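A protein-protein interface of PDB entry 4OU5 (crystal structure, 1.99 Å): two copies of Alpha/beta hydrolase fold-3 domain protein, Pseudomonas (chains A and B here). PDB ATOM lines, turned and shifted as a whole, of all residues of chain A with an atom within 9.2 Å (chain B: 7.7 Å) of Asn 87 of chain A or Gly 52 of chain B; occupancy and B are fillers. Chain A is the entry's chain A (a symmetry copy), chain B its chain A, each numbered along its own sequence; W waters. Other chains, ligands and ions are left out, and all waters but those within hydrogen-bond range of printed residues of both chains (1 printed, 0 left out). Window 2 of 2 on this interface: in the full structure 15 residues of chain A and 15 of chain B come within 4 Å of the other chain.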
ATOM      1  N   SER A  62     -12.213 -21.341  -1.818  1.00  0.00           N
ATOM      2  CA  SER A  62     -12.728 -21.590  -3.165  1.00  0.00           C
ATOM      3  C   SER A  62     -11.629 -21.831  -4.191  1.00  0.00           C
ATOM      4  O   SER A  62     -10.452 -21.559  -3.934  1.00  0.00           O
ATOM      5  CB  SER A  62     -13.585 -20.414  -3.633  1.00  0.00           C
ATOM      6  OG  SER A  62     -12.795 -19.249  -3.768  1.00  0.00           O
ATOM      7  N   GLY A  63     -12.027 -22.336  -5.359  1.00  0.00           N
ATOM      8  CA  GLY A  63     -11.129 -22.465  -6.499  1.00  0.00           C
ATOM      9  C   GLY A  63     -10.346 -23.771  -6.529  1.00  0.00           C
ATOM     10  O   GLY A  63      -9.437 -23.952  -7.344  1.00  0.00           O
ATOM     11  N   ILE A  64     -10.689 -24.688  -5.630  1.00  0.00           N
ATOM     12  CA  ILE A  64      -9.994 -25.963  -5.550  1.00  0.00           C
ATOM     13  C   ILE A  64     -10.991 -27.098  -5.493  1.00  0.00           C
ATOM     14  O   ILE A  64     -12.136 -26.916  -5.077  1.00  0.00           O
ATOM     15  CB  ILE A  64      -9.077 -26.053  -4.299  1.00  0.00           C
ATOM     16  CG1 ILE A  64      -9.901 -25.846  -3.024  1.00  0.00           C
ATOM     17  CG2 ILE A  64      -7.939 -25.043  -4.378  1.00  0.00           C
ATOM     18  CD1 ILE A  64      -9.155 -26.190  -1.738  1.00  0.00           C
ATOM     19  N   GLU A  65     -10.560 -28.279  -5.910  1.00  0.00           N
ATOM     20  CA  GLU A  65     -11.347 -29.471  -5.647  1.00  0.00           C
ATOM     21  C   GLU A  65     -10.466 -30.486  -4.930  1.00  0.00           C
ATOM     22  O   GLU A  65      -9.324 -30.751  -5.331  1.00  0.00           O
ATOM     23  CB  GLU A  65     -11.949 -30.045  -6.934  1.00  0.00           C
ATOM     24  CG  GLU A  65     -10.980 -30.606  -7.938  1.00  0.00           C
ATOM     25  CD  GLU A  65     -11.694 -31.136  -9.177  1.00  0.00           C
ATOM     26  OE1 GLU A  65     -11.970 -32.353  -9.235  1.00  0.00           O
ATOM     27  OE2 GLU A  65     -11.991 -30.326 -10.085  1.00  0.00           O
ATOM     28  N   ARG A  84      -6.721 -29.982  -6.299  1.00  0.00           N
ATOM     29  CA  ARG A  84      -6.580 -29.602  -7.706  1.00  0.00           C
ATOM     30  C   ARG A  84      -7.234 -28.248  -7.964  1.00  0.00           C
ATOM     31  O   ARG A  84      -8.309 -27.980  -7.414  1.00  0.00           O
ATOM     32  CB  ARG A  84      -7.218 -30.686  -8.595  1.00  0.00           C
ATOM     33  CG  ARG A  84      -7.093 -30.461 -10.090  1.00  0.00           C
ATOM     34  CD  ARG A  84      -7.987 -31.430 -10.873  1.00  0.00           C
ATOM     35  NE  ARG A  84      -7.911 -31.144 -12.304  1.00  0.00           N
ATOM     36  CZ  ARG A  84      -6.986 -31.649 -13.114  1.00  0.00           C
ATOM     37  NH1 ARG A  84      -6.070 -32.490 -12.642  1.00  0.00           N
ATOM     38  NH2 ARG A  84      -6.985 -31.321 -14.400  1.00  0.00           N
ATOM     39  N   PRO A  85      -6.591 -27.385  -8.778  1.00  0.00           N
ATOM     40  CA  PRO A  85      -7.281 -26.173  -9.245  1.00  0.00           C
ATOM     41  C   PRO A  85      -8.631 -26.540  -9.873  1.00  0.00           C
ATOM     42  O   PRO A  85      -8.697 -27.462 -10.685  1.00  0.00           O
ATOM     43  CB  PRO A  85      -6.320 -25.596 -10.289  1.00  0.00           C
ATOM     44  CG  PRO A  85      -4.965 -26.116  -9.892  1.00  0.00           C
ATOM     45  CD  PRO A  85      -5.217 -27.483  -9.309  1.00  0.00           C
ATOM     46  N   ALA A  86      -9.693 -25.843  -9.486  1.00  0.00           N
ATOM     47  CA  ALA A  86     -11.031 -26.197  -9.946  1.00  0.00           C
ATOM     48  C   ALA A  86     -11.234 -25.807 -11.406  1.00  0.00           C
ATOM     49  O   ALA A  86     -10.613 -24.862 -11.895  1.00  0.00           O
ATOM     50  CB  ALA A  86     -12.097 -25.527  -9.073  1.00  0.00           C
ATOM     51  N   ASN A  87     -12.117 -26.534 -12.077  1.00  0.00           N
ATOM     52  CA  ASN A  87     -12.527 -26.201 -13.436  1.00  0.00           C
ATOM     53  C   ASN A  87     -11.366 -26.179 -14.430  1.00  0.00           C
ATOM     54  O   ASN A  87     -11.319 -25.338 -15.326  1.00  0.00           O
ATOM     55  CB  ASN A  87     -13.257 -24.856 -13.433  1.00  0.00           C
ATOM     56  CG  ASN A  87     -14.564 -24.912 -12.656  1.00  0.00           C
ATOM     57  OD1 ASN A  87     -15.482 -25.638 -13.031  1.00  0.00           O
ATOM     58  ND2 ASN A  87     -14.644 -24.168 -11.560  1.00  0.00           N
ATOM     59  N   VAL A  88     -10.434 -27.113 -14.270  1.00  0.00           N
ATOM     60  CA  VAL A  88      -9.274 -27.210 -15.158  1.00  0.00           C
ATOM     61  C   VAL A  88      -9.139 -28.636 -15.674  1.00  0.00           C
ATOM     62  O   VAL A  88      -9.134 -29.593 -14.895  1.00  0.00           O
ATOM     63  CB  VAL A  88      -7.959 -26.793 -14.445  1.00  0.00           C
ATOM     64  CG1 VAL A  88      -6.742 -27.037 -15.358  1.00  0.00           C
ATOM     65  CG2 VAL A  88      -8.029 -25.334 -14.006  1.00  0.00           C
ATOM     66  N   LYS A  89      -9.031 -28.774 -16.991  1.00  0.00           N
ATOM     67  CA  LYS A  89      -8.940 -30.087 -17.621  1.00  0.00           C
ATOM     68  C   LYS A  89      -7.492 -30.443 -17.901  1.00  0.00           C
ATOM     69  O   LYS A  89      -6.657 -29.557 -18.091  1.00  0.00           O
ATOM     70  CB  LYS A  89      -9.739 -30.119 -18.930  1.00  0.00           C
ATOM     71  CG  LYS A  89     -11.207 -29.783 -18.774  1.00  0.00           C
ATOM     72  CD  LYS A  89     -12.042 -31.030 -18.593  1.00  0.00           C
ATOM     73  CE  LYS A  89     -13.516 -30.674 -18.455  1.00  0.00           C
ATOM     74  NZ  LYS A  89     -13.994 -29.795 -19.566  1.00  0.00           N
ATOM     75  N   GLY A  90      -7.209 -31.741 -17.935  1.00  0.00           N
ATOM     76  CA  GLY A  90      -5.915 -32.236 -18.369  1.00  0.00           C
ATOM     77  C   GLY A  90      -4.939 -32.498 -17.242  1.00  0.00           C
ATOM     78  O   GLY A  90      -5.219 -32.209 -16.077  1.00  0.00           O
ATOM     79  N   LEU A  92      -1.871 -31.860 -14.903  1.00  0.00           N
ATOM     80  CA  LEU A  92      -1.290 -30.653 -14.334  1.00  0.00           C
ATOM     81  C   LEU A  92      -0.003 -31.044 -13.633  1.00  0.00           C
ATOM     82  O   LEU A  92       0.116 -32.174 -13.153  1.00  0.00           O
ATOM     83  CB  LEU A  92      -2.265 -29.989 -13.347  1.00  0.00           C
ATOM     84  CG  LEU A  92      -3.516 -29.321 -13.924  1.00  0.00           C
ATOM     85  CD1 LEU A  92      -4.463 -28.820 -12.817  1.00  0.00           C
ATOM     86  CD2 LEU A  92      -3.104 -28.169 -14.835  1.00  0.00           C
ATOM     87  N   ALA B  46     -21.023 -35.159 -15.354  1.00  0.00           N
ATOM     88  CA  ALA B  46     -22.099 -34.525 -14.576  1.00  0.00           C
ATOM     89  C   ALA B  46     -21.624 -34.164 -13.160  1.00  0.00           C
ATOM     90  O   ALA B  46     -21.883 -33.064 -12.664  1.00  0.00           O
ATOM     91  CB  ALA B  46     -23.323 -35.443 -14.514  1.00  0.00           C
ATOM     92  N   ARG B  47     -20.928 -35.100 -12.518  1.00  0.00           N
ATOM     93  CA  ARG B  47     -20.329 -34.875 -11.202  1.00  0.00           C
ATOM     94  C   ARG B  47     -19.410 -33.652 -11.194  1.00  0.00           C
ATOM     95  O   ARG B  47     -19.450 -32.835 -10.267  1.00  0.00           O
ATOM     96  CB  ARG B  47     -19.552 -36.121 -10.756  1.00  0.00           C
ATOM     97  CG  ARG B  47     -20.460 -37.268 -10.381  1.00  0.00           C
ATOM     98  CD  ARG B  47     -19.778 -38.629 -10.377  1.00  0.00           C
ATOM     99  NE  ARG B  47     -20.797 -39.658 -10.204  1.00  0.00           N
ATOM    100  CZ  ARG B  47     -20.637 -40.950 -10.459  1.00  0.00           C
ATOM    101  NH1 ARG B  47     -19.471 -41.407 -10.912  1.00  0.00           N
ATOM    102  NH2 ARG B  47     -21.653 -41.781 -10.260  1.00  0.00           N
ATOM    103  N   ALA B  48     -18.599 -33.516 -12.240  1.00  0.00           N
ATOM    104  CA  ALA B  48     -17.686 -32.379 -12.345  1.00  0.00           C
ATOM    105  C   ALA B  48     -18.427 -31.033 -12.484  1.00  0.00           C
ATOM    106  O   ALA B  48     -17.906 -29.997 -12.082  1.00  0.00           O
ATOM    107  CB  ALA B  48     -16.726 -32.586 -13.519  1.00  0.00           C
ATOM    108  N   VAL B  49     -19.638 -31.038 -13.045  1.00  0.00           N
ATOM    109  CA  VAL B  49     -20.394 -29.788 -13.163  1.00  0.00           C
ATOM    110  C   VAL B  49     -20.676 -29.223 -11.776  1.00  0.00           C
ATOM    111  O   VAL B  49     -20.408 -28.054 -11.507  1.00  0.00           O
ATOM    112  CB  VAL B  49     -21.733 -29.970 -13.916  1.00  0.00           C
ATOM    113  CG1 VAL B  49     -22.543 -28.689 -13.860  1.00  0.00           C
ATOM    114  CG2 VAL B  49     -21.489 -30.377 -15.350  1.00  0.00           C
ATOM    115  N   LEU B  50     -21.194 -30.075 -10.895  1.00  0.00           N
ATOM    116  CA  LEU B  50     -21.486 -29.681  -9.525  1.00  0.00           C
ATOM    117  C   LEU B  50     -20.206 -29.308  -8.790  1.00  0.00           C
ATOM    118  O   LEU B  50     -20.151 -28.289  -8.118  1.00  0.00           O
ATOM    119  CB  LEU B  50     -22.210 -30.809  -8.776  1.00  0.00           C
ATOM    120  CG  LEU B  50     -22.507 -30.579  -7.285  1.00  0.00           C
ATOM    121  CD1 LEU B  50     -23.410 -29.361  -7.070  1.00  0.00           C
ATOM    122  CD2 LEU B  50     -23.133 -31.830  -6.655  1.00  0.00           C
ATOM    123  N   THR B  51     -19.177 -30.142  -8.913  1.00  0.00           N
ATOM    124  CA  THR B  51     -17.894 -29.856  -8.267  1.00  0.00           C
ATOM    125  C   THR B  51     -17.358 -28.475  -8.668  1.00  0.00           C
ATOM    126  O   THR B  51     -17.009 -27.657  -7.805  1.00  0.00           O
ATOM    127  CB  THR B  51     -16.846 -30.934  -8.604  1.00  0.00           C
ATOM    128  OG1 THR B  51     -17.232 -32.182  -8.008  1.00  0.00           O
ATOM    129  CG2 THR B  51     -15.456 -30.521  -8.108  1.00  0.00           C
ATOM    130  N   GLY B  52     -17.313 -28.211  -9.972  1.00  0.00           N
ATOM    131  CA  GLY B  52     -16.793 -26.951 -10.470  1.00  0.00           C
ATOM    132  C   GLY B  52     -17.620 -25.747 -10.052  1.00  0.00           C
ATOM    133  O   GLY B  52     -17.074 -24.696  -9.684  1.00  0.00           O
ATOM    134  N   ALA B  53     -18.941 -25.897 -10.104  1.00  0.00           N
ATOM    135  CA  ALA B  53     -19.848 -24.805  -9.752  1.00  0.00           C
ATOM    136  C   ALA B  53     -19.745 -24.458  -8.266  1.00  0.00           C
ATOM    137  O   ALA B  53     -19.724 -23.283  -7.891  1.00  0.00           O
ATOM    138  CB  ALA B  53     -21.297 -25.162 -10.120  1.00  0.00           C
ATOM    139  N   GLN B  54     -19.665 -25.480  -7.419  1.00  0.00           N
ATOM    140  CA  GLN B  54     -19.570 -25.242  -5.982  1.00  0.00           C
ATOM    141  C   GLN B  54     -18.242 -24.593  -5.605  1.00  0.00           C
ATOM    142  O   GLN B  54     -18.182 -23.775  -4.691  1.00  0.00           O
ATOM    143  CB  GLN B  54     -19.759 -26.554  -5.206  1.00  0.00           C
ATOM    144  CG  GLN B  54     -21.174 -27.147  -5.319  1.00  0.00           C
ATOM    145  CD  GLN B  54     -22.227 -26.269  -4.652  1.00  0.00           C
ATOM    146  OE1 GLN B  54     -22.638 -25.239  -5.198  1.00  0.00           O
ATOM    147  NE2 GLN B  54     -22.647 -26.660  -3.450  1.00  0.00           N
ATOM    148  N   ALA B  55     -17.182 -24.964  -6.311  1.00  0.00           N
ATOM    149  CA  ALA B  55     -15.829 -24.510  -5.983  1.00  0.00           C
ATOM    150  C   ALA B  55     -15.544 -23.089  -6.445  1.00  0.00           C
ATOM    151  O   ALA B  55     -14.543 -22.495  -6.063  1.00  0.00           O
ATOM    152  CB  ALA B  55     -14.802 -25.459  -6.591  1.00  0.00           C
ATOM    153  N   SER B  56     -16.418 -22.528  -7.265  1.00  0.00           N
ATOM    154  CA  SER B  56     -16.112 -21.247  -7.881  1.00  0.00           C
ATOM    155  C   SER B  56     -16.687 -20.087  -7.077  1.00  0.00           C
ATOM    156  O   SER B  56     -16.680 -18.945  -7.528  1.00  0.00           O
ATOM    157  CB  SER B  56     -16.647 -21.210  -9.307  1.00  0.00           C
ATOM    158  OG  SER B  56     -18.060 -21.186  -9.274  1.00  0.00           O
ATOM    159  N   VAL B  57     -17.191 -20.391  -5.886  1.00  0.00           N
ATOM    160  CA  VAL B  57     -17.826 -19.393  -5.043  1.00  0.00           C
ATOM    161  C   VAL B  57     -17.104 -19.296  -3.702  1.00  0.00           C
ATOM    162  O   VAL B  57     -16.926 -20.297  -3.014  1.00  0.00           O
ATOM    163  CB  VAL B  57     -19.324 -19.737  -4.793  1.00  0.00           C
ATOM    164  CG1 VAL B  57     -20.013 -18.603  -4.055  1.00  0.00           C
ATOM    165  CG2 VAL B  57     -20.038 -20.030  -6.110  1.00  0.00           C
ATOM    166  N   THR B 110     -18.789 -31.137  -2.230  1.00  0.00           N
ATOM    167  CA  THR B 110     -19.823 -30.338  -2.900  1.00  0.00           C
ATOM    168  C   THR B 110     -20.886 -29.859  -1.906  1.00  0.00           C
ATOM    169  O   THR B 110     -21.477 -28.791  -2.081  1.00  0.00           O
ATOM    170  CB  THR B 110     -20.551 -31.112  -4.035  1.00  0.00           C
ATOM    171  OG1 THR B 110     -21.056 -32.356  -3.534  1.00  0.00           O
ATOM    172  CG2 THR B 110     -19.621 -31.367  -5.247  1.00  0.00           C
HETATM  173  O   HOH W   1     -17.957 -24.327 -12.947  1.00  0.00           O
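No position is printed for both chains. Of the 7 pairs that touch across the chains among the printed residues, none has its exchanged pair printed and touching as well.
Printed residues of chain A that touch a printed residue of chain B: Ser 62, Gly 63, Ile 64, Glu 65, Ala 86 and Asn 87. Along chain A the printed residues that touch a printed residue of chain B span positions 62 to 87. Of the 13 printed residues of chain B, 4 touch a printed residue of chain A. Printed residues of chain B that touch a printed residue of chain A: Thr 51, Gly 52, Ala 55 and Val 57. Along chain B the printed residues that touch a printed residue of chain A span positions 51 to 57. Among the printed residues, no Asp or Glu carboxylate lies within 4 Å of a Lys or Arg side-chain nitrogen of the other chain.
Printed residues of chain B within 4 Å of Ser 62 of chain A: Ala 55 (3.3 Å) and Val 57 (3.4 Å). Printed residues of chain B within 4 Å of Glu 65 of chain A: Thr 51 (3.7 Å). Of chain B, only Ala 55 comes within 4 Å of Ala 86 of chain A. Of chain B, only Gly 52 comes within 4 Å of Asn 87 of chain A. Printed residues of chain A within 4 Å of Thr 51 of chain B: Glu 65 (3.7 Å). No residue of chain A comes within 4 Å of Ala 53 of chain B. Ala 55 of chain B touches just these residues of chain A: Ser 62 (3.3 Å), Gly 63 (2.6 Å), Ile 64 (3.4 Å) and Ala 86 (3.7 Å). The nearest residue of chain B that does not touch Asn 87 of chain A is Ser 56 of chain B (4.2 Å). The nearest printed residue of chain B that does not touch Ile 64 of chain A is Thr 51 of chain B (5.6 Å).
Among the printed residues, pairs that only touch across the chains: Ser 62 of chain A with Ala 55 of chain B (3.3 Å), Ile 64 of chain A with Ala 55 of chain B (3.4 Å), Ser 62 of chain A with Val 57 of chain B (3.4 Å), Ala 86 of chain A with Ala 55 of chain B (3.7 Å) and Glu 65 of chain A with Thr 51 of chain B (3.7 Å).
Water W1 lies within hydrogen-bond range of the side-chain amide oxygen (OD1) of Asn 87 of chain A (2.8 Å), the backbone NH (N) of Ala 53 of chain B (3.4 Å) and the backbone carbonyl oxygen (O) of Gly 52 of chain B (3.4 Å).
OG1 of Thr 51 of chain B lies within hydrogen-bond range of O of Arg 47 of chain B, 3.2 Å away. The backbone NH (N) of Ala 86 of chain A is in hydrogen-bond range of the backbone carbonyl oxygen (O) of Gly 63 of chain A, at 2.9 Å. The backbone carbonyl oxygen (O) of Arg 84 of chain A lies within hydrogen-bond range of the backbone NH (N) of Glu 65 of chain A (2.7 Å).
The side-chain amide nitrogen (ND2) of Asn 87 of chain A sits at hydrogen-bond distance from the backbone carbonyl oxygen (O) of Gly 52 of chain B, at 3.1 Å. O of Ala 55 of chain B is in hydrogen-bond range of N of Gly 63 of chain A, 2.6 Å away.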
